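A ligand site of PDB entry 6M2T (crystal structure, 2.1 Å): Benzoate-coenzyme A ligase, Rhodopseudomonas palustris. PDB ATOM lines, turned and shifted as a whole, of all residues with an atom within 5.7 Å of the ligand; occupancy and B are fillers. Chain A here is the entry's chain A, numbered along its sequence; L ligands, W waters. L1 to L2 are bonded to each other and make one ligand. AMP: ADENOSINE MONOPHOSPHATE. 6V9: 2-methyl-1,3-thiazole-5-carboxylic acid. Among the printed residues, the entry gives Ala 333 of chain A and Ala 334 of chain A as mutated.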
ATOM      1  N   SER A 181      -9.817  12.567  26.117  1.00  0.00           N
ATOM      2  CA  SER A 181     -10.230  11.161  26.199  1.00  0.00           C
ATOM      3  C   SER A 181     -10.446  10.785  27.665  1.00  0.00           C
ATOM      4  O   SER A 181      -9.678  11.191  28.544  1.00  0.00           O
ATOM      5  CB  SER A 181      -9.161  10.255  25.571  1.00  0.00           C
ATOM      6  OG  SER A 181      -9.533   8.878  25.641  1.00  0.00           O
ATOM      7  N   PHE A 226     -13.294  13.686  17.042  1.00  0.00           N
ATOM      8  CA  PHE A 226     -12.698  12.374  17.292  1.00  0.00           C
ATOM      9  C   PHE A 226     -11.380  12.234  16.526  1.00  0.00           C
ATOM     10  O   PHE A 226     -11.296  12.595  15.357  1.00  0.00           O
ATOM     11  CB  PHE A 226     -13.620  11.249  16.847  1.00  0.00           C
ATOM     12  CG  PHE A 226     -14.837  11.029  17.721  1.00  0.00           C
ATOM     13  CD1 PHE A 226     -14.709  10.605  19.040  1.00  0.00           C
ATOM     14  CD2 PHE A 226     -16.121  11.228  17.194  1.00  0.00           C
ATOM     15  CE1 PHE A 226     -15.836  10.390  19.829  1.00  0.00           C
ATOM     16  CE2 PHE A 226     -17.263  11.015  17.974  1.00  0.00           C
ATOM     17  CZ  PHE A 226     -17.119  10.603  19.291  1.00  0.00           C
ATOM     18  N   ALA A 227     -10.366  11.682  17.190  1.00  0.00           N
ATOM     19  CA  ALA A 227      -9.107  11.388  16.508  1.00  0.00           C
ATOM     20  C   ALA A 227      -9.343  10.696  15.183  1.00  0.00           C
ATOM     21  O   ALA A 227      -8.763  11.059  14.150  1.00  0.00           O
ATOM     22  CB  ALA A 227      -8.211  10.537  17.420  1.00  0.00           C
ATOM     23  N   TYR A 228     -10.229   9.694  15.176  1.00  0.00           N
ATOM     24  CA  TYR A 228     -10.551   8.976  13.946  1.00  0.00           C
ATOM     25  C   TYR A 228     -11.074   9.946  12.883  1.00  0.00           C
ATOM     26  O   TYR A 228     -10.576   9.984  11.757  1.00  0.00           O
ATOM     27  CB  TYR A 228     -11.567   7.872  14.276  1.00  0.00           C
ATOM     28  CG  TYR A 228     -12.000   6.938  13.164  1.00  0.00           C
ATOM     29  CD1 TYR A 228     -11.071   6.368  12.281  1.00  0.00           C
ATOM     30  CD2 TYR A 228     -13.334   6.578  13.024  1.00  0.00           C
ATOM     31  CE1 TYR A 228     -11.498   5.485  11.268  1.00  0.00           C
ATOM     32  CE2 TYR A 228     -13.770   5.712  12.031  1.00  0.00           C
ATOM     33  CZ  TYR A 228     -12.859   5.166  11.169  1.00  0.00           C
ATOM     34  OH  TYR A 228     -13.321   4.305  10.207  1.00  0.00           O
ATOM     35  N   ASN A 232      -9.731  11.057   9.072  1.00  0.00           N
ATOM     36  CA  ASN A 232     -10.573  10.667   7.946  1.00  0.00           C
ATOM     37  C   ASN A 232     -10.981  11.858   7.106  1.00  0.00           C
ATOM     38  O   ASN A 232     -11.033  11.782   5.878  1.00  0.00           O
ATOM     39  CB  ASN A 232     -11.844   9.955   8.436  1.00  0.00           C
ATOM     40  CG  ASN A 232     -11.573   8.797   9.413  1.00  0.00           C
ATOM     41  OD1 ASN A 232     -10.514   8.161   9.385  1.00  0.00           O
ATOM     42  ND2 ASN A 232     -12.559   8.508  10.256  1.00  0.00           N
ATOM     43  N   SER A 301     -13.526   1.184   9.041  1.00  0.00           N
ATOM     44  CA  SER A 301     -14.230   1.033  10.309  1.00  0.00           C
ATOM     45  C   SER A 301     -13.249   1.141  11.470  1.00  0.00           C
ATOM     46  O   SER A 301     -12.106   0.676  11.376  1.00  0.00           O
ATOM     47  CB  SER A 301     -14.970  -0.309  10.387  1.00  0.00           C
ATOM     48  OG  SER A 301     -15.670  -0.419  11.605  1.00  0.00           O
ATOM     49  N   ALA A 302     -13.703   1.733  12.580  1.00  0.00           N
ATOM     50  CA  ALA A 302     -12.885   1.798  13.790  1.00  0.00           C
ATOM     51  C   ALA A 302     -13.768   2.121  14.993  1.00  0.00           C
ATOM     52  O   ALA A 302     -14.932   2.493  14.849  1.00  0.00           O
ATOM     53  CB  ALA A 302     -11.768   2.844  13.655  1.00  0.00           C
ATOM     54  N   GLY A 303     -13.169   2.009  16.185  1.00  0.00           N
ATOM     55  CA  GLY A 303     -13.785   2.409  17.435  1.00  0.00           C
ATOM     56  C   GLY A 303     -14.146   1.237  18.334  1.00  0.00           C
ATOM     57  O   GLY A 303     -14.062   1.372  19.560  1.00  0.00           O
ATOM     58  N   GLU A 304     -14.528   0.117  17.741  1.00  0.00           N
ATOM     59  CA  GLU A 304     -14.858  -1.136  18.388  1.00  0.00           C
ATOM     60  C   GLU A 304     -14.528  -2.222  17.379  1.00  0.00           C
ATOM     61  O   GLU A 304     -14.425  -1.944  16.170  1.00  0.00           O
ATOM     62  CB  GLU A 304     -16.333  -1.183  18.793  1.00  0.00           C
ATOM     63  CG  GLU A 304     -17.288  -1.087  17.589  1.00  0.00           C
ATOM     64  CD  GLU A 304     -18.730  -0.767  17.980  1.00  0.00           C
ATOM     65  OE1 GLU A 304     -19.108  -1.077  19.133  1.00  0.00           O
ATOM     66  OE2 GLU A 304     -19.466  -0.186  17.161  1.00  0.00           O
ATOM     67  N   ALA A 305     -14.345  -3.451  17.860  1.00  0.00           N
ATOM     68  CA  ALA A 305     -14.134  -4.587  16.957  1.00  0.00           C
ATOM     69  C   ALA A 305     -15.288  -4.698  15.954  1.00  0.00           C
ATOM     70  O   ALA A 305     -16.457  -4.540  16.313  1.00  0.00           O
ATOM     71  CB  ALA A 305     -14.009  -5.902  17.732  1.00  0.00           C
ATOM     72  N   LEU A 306     -14.947  -4.986  14.698  1.00  0.00           N
ATOM     73  CA  LEU A 306     -15.935  -5.248  13.658  1.00  0.00           C
ATOM     74  C   LEU A 306     -16.373  -6.707  13.712  1.00  0.00           C
ATOM     75  O   LEU A 306     -15.572  -7.591  13.388  1.00  0.00           O
ATOM     76  CB  LEU A 306     -15.388  -4.935  12.267  1.00  0.00           C
ATOM     77  CG  LEU A 306     -16.317  -5.275  11.085  1.00  0.00           C
ATOM     78  CD1 LEU A 306     -17.465  -4.295  11.025  1.00  0.00           C
ATOM     79  CD2 LEU A 306     -15.550  -5.286   9.764  1.00  0.00           C
ATOM     80  N   ASP A 324     -11.157  -2.840   8.772  1.00  0.00           N
ATOM     81  CA  ASP A 324     -11.223  -2.597  10.216  1.00  0.00           C
ATOM     82  C   ASP A 324      -9.813  -2.316  10.713  1.00  0.00           C
ATOM     83  O   ASP A 324      -8.900  -3.123  10.513  1.00  0.00           O
ATOM     84  CB  ASP A 324     -11.830  -3.837  10.887  1.00  0.00           C
ATOM     85  CG  ASP A 324     -11.812  -3.793  12.418  1.00  0.00           C
ATOM     86  OD1 ASP A 324     -11.623  -2.711  13.010  1.00  0.00           O
ATOM     87  OD2 ASP A 324     -12.020  -4.874  13.027  1.00  0.00           O
ATOM     88  N   GLY A 325      -9.608  -1.136  11.294  1.00  0.00           N
ATOM     89  CA  GLY A 325      -8.335  -0.808  11.918  1.00  0.00           C
ATOM     90  C   GLY A 325      -8.575  -0.269  13.318  1.00  0.00           C
ATOM     91  O   GLY A 325      -9.639   0.257  13.628  1.00  0.00           O
ATOM     92  N   ILE A 326      -7.567  -0.415  14.179  1.00  0.00           N
ATOM     93  CA  ILE A 326      -7.674   0.071  15.543  1.00  0.00           C
ATOM     94  C   ILE A 326      -6.685   1.202  15.714  1.00  0.00           C
ATOM     95  O   ILE A 326      -5.483   1.039  15.465  1.00  0.00           O
ATOM     96  CB  ILE A 326      -7.431  -1.023  16.601  1.00  0.00           C
ATOM     97  CG1 ILE A 326      -7.496  -0.386  18.001  1.00  0.00           C
ATOM     98  CG2 ILE A 326      -6.109  -1.751  16.399  1.00  0.00           C
ATOM     99  CD1 ILE A 326      -7.131  -1.335  19.141  1.00  0.00           C
ATOM    100  N   GLY A 327      -7.205   2.353  16.122  1.00  0.00           N
ATOM    101  CA  GLY A 327      -6.374   3.451  16.582  1.00  0.00           C
ATOM    102  C   GLY A 327      -6.769   3.881  17.991  1.00  0.00           C
ATOM    103  O   GLY A 327      -7.583   3.228  18.638  1.00  0.00           O
ATOM    104  N   SER A 328      -6.189   4.972  18.473  1.00  0.00           N
ATOM    105  CA  SER A 328      -6.574   5.534  19.750  1.00  0.00           C
ATOM    106  C   SER A 328      -6.300   7.036  19.715  1.00  0.00           C
ATOM    107  O   SER A 328      -5.558   7.533  18.872  1.00  0.00           O
ATOM    108  CB  SER A 328      -5.799   4.873  20.898  1.00  0.00           C
ATOM    109  OG  SER A 328      -4.429   5.252  20.826  1.00  0.00           O
ATOM    110  N   THR A 329      -6.921   7.748  20.661  1.00  0.00           N
ATOM    111  CA  THR A 329      -6.652   9.182  20.767  1.00  0.00           C
ATOM    112  C   THR A 329      -5.167   9.424  21.020  1.00  0.00           C
ATOM    113  O   THR A 329      -4.554  10.312  20.412  1.00  0.00           O
ATOM    114  CB  THR A 329      -7.538   9.812  21.848  1.00  0.00           C
ATOM    115  OG1 THR A 329      -8.915   9.536  21.559  1.00  0.00           O
ATOM    116  CG2 THR A 329      -7.338  11.321  21.896  1.00  0.00           C
ATOM    117  N   GLU A 330      -4.558   8.594  21.887  1.00  0.00           N
ATOM    118  CA  GLU A 330      -3.138   8.740  22.185  1.00  0.00           C
ATOM    119  C   GLU A 330      -2.225   8.462  20.980  1.00  0.00           C
ATOM    120  O   GLU A 330      -1.198   9.128  20.812  1.00  0.00           O
ATOM    121  CB  GLU A 330      -2.753   7.817  23.344  1.00  0.00           C
ATOM    122  CG  GLU A 330      -3.385   8.228  24.665  1.00  0.00           C
ATOM    123  CD  GLU A 330      -4.769   7.603  24.900  1.00  0.00           C
ATOM    124  OE1 GLU A 330      -5.387   7.085  23.944  1.00  0.00           O
ATOM    125  OE2 GLU A 330      -5.245   7.640  26.045  1.00  0.00           O
ATOM    126  N   LEU A 332      -3.368   8.736  17.811  1.00  0.00           N
ATOM    127  CA  LEU A 332      -3.975   9.585  16.784  1.00  0.00           C
ATOM    128  C   LEU A 332      -4.630   8.825  15.631  1.00  0.00           C
ATOM    129  O   LEU A 332      -5.736   9.197  15.223  1.00  0.00           O
ATOM    130  CB  LEU A 332      -2.970  10.601  16.224  1.00  0.00           C
ATOM    131  CG  LEU A 332      -3.542  11.704  15.313  1.00  0.00           C
ATOM    132  CD1 LEU A 332      -4.658  12.489  15.994  1.00  0.00           C
ATOM    133  CD2 LEU A 332      -2.460  12.686  14.850  1.00  0.00           C
ATOM    134  N   ALA A 333      -4.006   7.775  15.087  1.00  0.00           N
ATOM    135  CA  ALA A 333      -4.691   6.980  14.057  1.00  0.00           C
ATOM    136  C   ALA A 333      -4.328   5.506  14.230  1.00  0.00           C
ATOM    137  O   ALA A 333      -3.717   5.101  15.224  1.00  0.00           O
ATOM    138  CB  ALA A 333      -4.386   7.478  12.645  1.00  0.00           C
ATOM    139  N   ALA A 334      -4.710   4.702  13.244  1.00  0.00           N
ATOM    140  CA  ALA A 334      -4.598   3.249  13.370  1.00  0.00           C
ATOM    141  C   ALA A 334      -3.144   2.803  13.390  1.00  0.00           C
ATOM    142  O   ALA A 334      -2.303   3.306  12.633  1.00  0.00           O
ATOM    143  CB  ALA A 334      -5.365   2.545  12.233  1.00  0.00           C
ATOM    144  N   PHE A 335      -2.847   1.826  14.254  1.00  0.00           N
ATOM    145  CA  PHE A 335      -1.542   1.178  14.313  1.00  0.00           C
ATOM    146  C   PHE A 335      -1.592  -0.304  13.997  1.00  0.00           C
ATOM    147  O   PHE A 335      -0.544  -0.906  13.759  1.00  0.00           O
ATOM    148  CB  PHE A 335      -0.926   1.389  15.703  1.00  0.00           C
ATOM    149  CG  PHE A 335      -1.915   1.212  16.825  1.00  0.00           C
ATOM    150  CD1 PHE A 335      -2.313  -0.069  17.216  1.00  0.00           C
ATOM    151  CD2 PHE A 335      -2.455   2.307  17.475  1.00  0.00           C
ATOM    152  CE1 PHE A 335      -3.228  -0.252  18.245  1.00  0.00           C
ATOM    153  CE2 PHE A 335      -3.381   2.140  18.514  1.00  0.00           C
ATOM    154  CZ  PHE A 335      -3.757   0.862  18.904  1.00  0.00           C
ATOM    155  N   THR A 348      -8.146  -7.609  13.664  1.00  0.00           N
ATOM    156  CA  THR A 348      -7.805  -6.245  13.296  1.00  0.00           C
ATOM    157  C   THR A 348      -6.604  -6.182  12.354  1.00  0.00           C
ATOM    158  O   THR A 348      -5.959  -5.126  12.233  1.00  0.00           O
ATOM    159  CB  THR A 348      -7.558  -5.385  14.538  1.00  0.00           C
ATOM    160  OG1 THR A 348      -8.370  -5.851  15.614  1.00  0.00           O
ATOM    161  CG2 THR A 348      -7.913  -3.914  14.244  1.00  0.00           C
ATOM    162  N   SER A 404      -2.043   0.675  25.497  1.00  0.00           N
ATOM    163  CA  SER A 404      -3.327   0.915  24.839  1.00  0.00           C
ATOM    164  C   SER A 404      -4.524   0.671  25.753  1.00  0.00           C
ATOM    165  O   SER A 404      -5.587   1.238  25.521  1.00  0.00           O
ATOM    166  CB  SER A 404      -3.472   0.015  23.612  1.00  0.00           C
ATOM    167  OG  SER A 404      -3.743  -1.324  24.007  1.00  0.00           O
ATOM    168  N   GLY A 405      -4.395  -0.196  26.764  1.00  0.00           N
ATOM    169  CA  GLY A 405      -5.543  -0.609  27.546  1.00  0.00           C
ATOM    170  C   GLY A 405      -6.254  -1.829  27.031  1.00  0.00           C
ATOM    171  O   GLY A 405      -7.246  -2.250  27.635  1.00  0.00           O
ATOM    172  N   ASP A 406      -5.784  -2.410  25.931  1.00  0.00           N
ATOM    173  CA  ASP A 406      -6.371  -3.575  25.288  1.00  0.00           C
ATOM    174  C   ASP A 406      -5.521  -4.817  25.485  1.00  0.00           C
ATOM    175  O   ASP A 406      -4.298  -4.745  25.684  1.00  0.00           O
ATOM    176  CB  ASP A 406      -6.531  -3.328  23.773  1.00  0.00           C
ATOM    177  CG  ASP A 406      -7.329  -2.083  23.453  1.00  0.00           C
ATOM    178  OD1 ASP A 406      -8.517  -2.000  23.852  1.00  0.00           O
ATOM    179  OD2 ASP A 406      -6.766  -1.179  22.806  1.00  0.00           O
ATOM    180  N   TYR A 408      -4.709  -8.367  23.269  1.00  0.00           N
ATOM    181  CA  TYR A 408      -4.775  -8.902  21.925  1.00  0.00           C
ATOM    182  C   TYR A 408      -4.063 -10.246  21.870  1.00  0.00           C
ATOM    183  O   TYR A 408      -3.192 -10.549  22.679  1.00  0.00           O
ATOM    184  CB  TYR A 408      -4.128  -7.954  20.904  1.00  0.00           C
ATOM    185  CG  TYR A 408      -5.086  -7.091  20.144  1.00  0.00           C
ATOM    186  CD1 TYR A 408      -5.564  -5.901  20.680  1.00  0.00           C
ATOM    187  CD2 TYR A 408      -5.514  -7.454  18.867  1.00  0.00           C
ATOM    188  CE1 TYR A 408      -6.443  -5.093  19.977  1.00  0.00           C
ATOM    189  CE2 TYR A 408      -6.388  -6.654  18.144  1.00  0.00           C
ATOM    190  CZ  TYR A 408      -6.853  -5.481  18.709  1.00  0.00           C
ATOM    191  OH  TYR A 408      -7.712  -4.684  17.995  1.00  0.00           O
ATOM    192  N   TYR A 418      -8.717  -9.055  18.721  1.00  0.00           N
ATOM    193  CA  TYR A 418      -9.034  -8.334  19.953  1.00  0.00           C
ATOM    194  C   TYR A 418      -9.507  -9.296  21.036  1.00  0.00           C
ATOM    195  O   TYR A 418     -10.311 -10.209  20.783  1.00  0.00           O
ATOM    196  CB  TYR A 418     -10.100  -7.278  19.678  1.00  0.00           C
ATOM    197  CG  TYR A 418     -10.591  -6.520  20.898  1.00  0.00           C
ATOM    198  CD1 TYR A 418      -9.826  -5.509  21.483  1.00  0.00           C
ATOM    199  CD2 TYR A 418     -11.854  -6.788  21.435  1.00  0.00           C
ATOM    200  CE1 TYR A 418     -10.296  -4.806  22.592  1.00  0.00           C
ATOM    201  CE2 TYR A 418     -12.330  -6.077  22.535  1.00  0.00           C
ATOM    202  CZ  TYR A 418     -11.548  -5.090  23.108  1.00  0.00           C
ATOM    203  OH  TYR A 418     -12.030  -4.407  24.199  1.00  0.00           O
ATOM    204  N   ARG A 421     -10.555  -5.419  27.086  1.00  0.00           N
ATOM    205  CA  ARG A 421      -9.841  -4.361  27.783  1.00  0.00           C
ATOM    206  C   ARG A 421      -9.202  -4.888  29.056  1.00  0.00           C
ATOM    207  O   ARG A 421      -9.530  -5.964  29.552  1.00  0.00           O
ATOM    208  CB  ARG A 421     -10.769  -3.189  28.151  1.00  0.00           C
ATOM    209  CG  ARG A 421     -11.510  -2.506  27.021  1.00  0.00           C
ATOM    210  CD  ARG A 421     -10.714  -1.354  26.421  1.00  0.00           C
ATOM    211  NE  ARG A 421     -10.269  -0.346  27.382  1.00  0.00           N
ATOM    212  CZ  ARG A 421      -9.357   0.597  27.099  1.00  0.00           C
ATOM    213  NH1 ARG A 421      -8.812   0.647  25.879  1.00  0.00           N
ATOM    214  NH2 ARG A 421      -8.972   1.478  28.014  1.00  0.00           N
ATOM    215  N   LYS A 427     -16.601   0.108  25.015  1.00  0.00           N
ATOM    216  CA  LYS A 427     -16.725   0.826  23.744  1.00  0.00           C
ATOM    217  C   LYS A 427     -18.109   0.504  23.195  1.00  0.00           C
ATOM    218  O   LYS A 427     -18.370  -0.635  22.787  1.00  0.00           O
ATOM    219  CB  LYS A 427     -15.634   0.435  22.761  1.00  0.00           C
ATOM    220  CG  LYS A 427     -14.371   1.259  22.891  1.00  0.00           C
ATOM    221  CD  LYS A 427     -14.719   2.739  22.857  1.00  0.00           C
ATOM    222  CE  LYS A 427     -13.494   3.598  22.518  1.00  0.00           C
ATOM    223  NZ  LYS A 427     -13.262   3.692  21.053  1.00  0.00           N
ATOM    224  N   GLY A 430     -18.675   2.317  19.285  1.00  0.00           N
ATOM    225  CA  GLY A 430     -17.304   2.737  19.082  1.00  0.00           C
ATOM    226  C   GLY A 430     -16.830   3.903  19.930  1.00  0.00           C
ATOM    227  O   GLY A 430     -15.768   4.475  19.622  1.00  0.00           O
ATOM    228  N   TYR A 432     -16.073   5.511  23.945  1.00  0.00           N
ATOM    229  CA  TYR A 432     -15.796   5.142  25.335  1.00  0.00           C
ATOM    230  C   TYR A 432     -16.991   5.414  26.225  1.00  0.00           C
ATOM    231  O   TYR A 432     -17.583   6.491  26.166  1.00  0.00           O
ATOM    232  CB  TYR A 432     -14.597   5.933  25.869  1.00  0.00           C
ATOM    233  CG  TYR A 432     -13.238   5.293  25.666  1.00  0.00           C
ATOM    234  CD1 TYR A 432     -13.049   3.928  25.857  1.00  0.00           C
ATOM    235  CD2 TYR A 432     -12.146   6.059  25.284  1.00  0.00           C
ATOM    236  CE1 TYR A 432     -11.816   3.346  25.679  1.00  0.00           C
ATOM    237  CE2 TYR A 432     -10.891   5.480  25.105  1.00  0.00           C
ATOM    238  CZ  TYR A 432     -10.722   4.126  25.297  1.00  0.00           C
ATOM    239  OH  TYR A 432      -9.486   3.558  25.119  1.00  0.00           O
HETATM  240  P   AMP L   1     -10.355   6.022  21.369  1.00  0.00           P
HETATM  241  O1P AMP L   1      -9.858   6.096  19.801  1.00  0.00           O
HETATM  242  O2P AMP L   1     -11.668   6.705  21.610  1.00  0.00           O
HETATM  243  O3P AMP L   1      -9.150   6.674  22.224  1.00  0.00           O
HETATM  244  O5' AMP L   1     -10.483   4.464  21.788  1.00  0.00           O
HETATM  245  C5' AMP L   1      -9.432   3.533  21.612  1.00  0.00           C
HETATM  246  C4' AMP L   1      -9.978   2.148  21.991  1.00  0.00           C
HETATM  247  O4' AMP L   1     -11.151   1.822  21.212  1.00  0.00           O
HETATM  248  C3' AMP L   1      -8.968   1.084  21.598  1.00  0.00           C
HETATM  249  O3' AMP L   1      -7.920   1.084  22.587  1.00  0.00           O
HETATM  250  C2' AMP L   1      -9.837  -0.142  21.702  1.00  0.00           C
HETATM  251  O2' AMP L   1     -10.263  -0.333  23.056  1.00  0.00           O
HETATM  252  C1' AMP L   1     -11.031   0.374  20.867  1.00  0.00           C
HETATM  253  N9  AMP L   1     -10.931   0.253  19.381  1.00  0.00           N
HETATM  254  C8  AMP L   1     -10.798   1.169  18.415  1.00  0.00           C
HETATM  255  N7  AMP L   1     -10.784   0.551  17.228  1.00  0.00           N
HETATM  256  C5  AMP L   1     -10.900  -0.760  17.454  1.00  0.00           C
HETATM  257  C6  AMP L   1     -10.952  -1.813  16.614  1.00  0.00           C
HETATM  258  N6  AMP L   1     -10.850  -1.558  15.305  1.00  0.00           N
HETATM  259  N1  AMP L   1     -11.083  -3.067  17.071  1.00  0.00           N
HETATM  260  C2  AMP L   1     -11.167  -3.274  18.449  1.00  0.00           C
HETATM  261  N3  AMP L   1     -11.126  -2.169  19.309  1.00  0.00           N
HETATM  262  C4  AMP L   1     -10.995  -0.937  18.782  1.00  0.00           C
HETATM  263  C1  6V9 L   2      -8.597   6.019  15.323  1.00  0.00           C
HETATM  264  C2  6V9 L   2      -7.996   6.114  13.920  1.00  0.00           C
HETATM  265  C   6V9 L   2     -10.341   5.358  18.740  1.00  0.00           C
HETATM  266  O   6V9 L   2     -11.268   4.544  18.843  1.00  0.00           O
HETATM  267  C3  6V9 L   2      -9.708   5.653  17.564  1.00  0.00           C
HETATM  268  S   6V9 L   2      -9.612   4.798  15.954  1.00  0.00           S
HETATM  269  N   6V9 L   2      -8.386   6.974  16.246  1.00  0.00           N
HETATM  270  C21 6V9 L   2      -8.984   6.789  17.459  1.00  0.00           C
HETATM  271  O   HOH W   1      -6.070   3.119  23.949  1.00  0.00           O
HETATM  272  O   HOH W   2     -13.735  -1.411  13.537  1.00  0.00           O
HETATM  273  O   HOH W   3     -11.625   8.624  17.898  1.00  0.00           O
HETATM  274  O   HOH W   4     -11.424   8.963  23.122  1.00  0.00           O
HETATM  275  O   HOH W   5     -14.320   7.693  22.798  1.00  0.00           O
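CB of Ala 227 touches N of 6V9 L2, at 3.8 Å. CB of Ala 302 touches S of 6V9 L2, at 3.7 Å. O of Glu 304 touches C6 of AMP L1 (3.5 Å). CG1 of Ile 326 touches C5 of AMP L1 (3.5 Å). CA of Ser 328 touches O1P of AMP L1, 3.3 Å away. O of Leu 332 touches N of 6V9 L2, 3.6 Å away. CA of Ala 333 touches C2 of 6V9 L2, at 3.4 Å. N of Ala 334 touches C2 of 6V9 L2, 3.6 Å away. CG2 of Thr 348 touches N6 of AMP L1 (3.9 Å). Ser 404 touches the ligand. Tyr 408 touches the ligand. CD1 of Tyr 418 touches C2 of AMP L1 (3.9998 Å). Tyr 432 touches the ligand. Hydrophobic or aromatic side chains within 4 Å of the ligand: Ala 227, Tyr 228, Ala 302, Ala 305, Ile 326, Tyr 418 and Tyr 432. Of the 32 residues printed, 23 come within 4 Å of the ligand. The nearest printed residue that does not touch the ligand is Ser 181 (4.1 Å).
The side-chain hydroxyl of Ser 404 is in hydrogen-bond range of the backbone NH of Asp 406. O of Tyr 228 sits close to ND2 of Asn 232 (2.9 Å). The backbone NH (N) of Gly 325 sits at hydrogen-bond distance from the backbone carbonyl oxygen (O) of Ser 301, 3.1 Å away. The backbone carbonyl oxygen (O) of Ile 326 is in hydrogen-bond range of the backbone NH (N) of Phe 335 (3.0 Å). N of Ser 301 sits at hydrogen-bond distance from OH of Tyr 228 (3.3 Å). The side-chain hydroxyl (OH) of Tyr 408 sits at hydrogen-bond distance from the side-chain hydroxyl (OG1) of Thr 348 (2.7 Å). The backbone NH of Leu 306 is in hydrogen-bond range of the side-chain carboxylate of Asp 324 (3.4 Å). The side-chain carboxylate (OE2) of Glu 304 sits close to the backbone NH (N) of Gly 430 (3.4 Å).
O of Gly 325 is in hydrogen-bond range of N6 of AMP L1 (2.8 Å). The backbone NH of Tyr 228 is in hydrogen-bond range of a nitrogen (N) of 6V9 L2, 3.5 Å away. NH1 of Arg 421 sits at hydrogen-bond distance from O2' of AMP L1. N of Gly 303 is in hydrogen-bond range of N7 of AMP L1 (3.0 Å). The side-chain carboxylate (OD1) of Asp 324 lies within hydrogen-bond range of a nitrogen (N6) of AMP L1. The backbone NH of Ala 305 sits close to a nitrogen (N1) of AMP L1 (3.4 Å). N of Gly 327 sits close to S of 6V9 L2, at 3.4 Å. An oxygen (O4') of AMP L1 is in hydrogen-bond range of the side-chain amino group (NZ) of Lys 427. The side-chain hydroxyl of Thr 329 is in hydrogen-bond range of an oxygen (O3P) of AMP L1 (2.9 Å). The side-chain carboxylate (OD1) of Asp 406 lies within hydrogen-bond range of an oxygen (O2') of AMP L1, at 2.5 Å. O3P of AMP L1 is in hydrogen-bond range of N of Thr 329, at 2.9 Å.
Water W4 lies within hydrogen-bond range of O2P of AMP L1 (2.7 Å), OG1 of Thr 329 (3.0 Å) and OG of Ser 181 (3.2 Å). Water W5 bridges the backbone NH of Tyr 432 (3.0 Å) and an oxygen (O2P) of AMP L1 (3.1 Å). Water W1 bridges the backbone carbonyl oxygen (O) of Ser 404 (2.5 Å) and an oxygen (O3') of AMP L1 (3.1 Å). Water W2 lies within hydrogen-bond range of the side-chain carboxylate (OD1) of Asp 324 (2.5 Å), the backbone carbonyl oxygen (O) of Glu 304 (2.8 Å), the side-chain hydroxyl (OG) of Ser 301 (2.9 Å), the backbone NH (N) of Ala 302 (3.3 Å) and a nitrogen (N6) of AMP L1 (3.4 Å).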
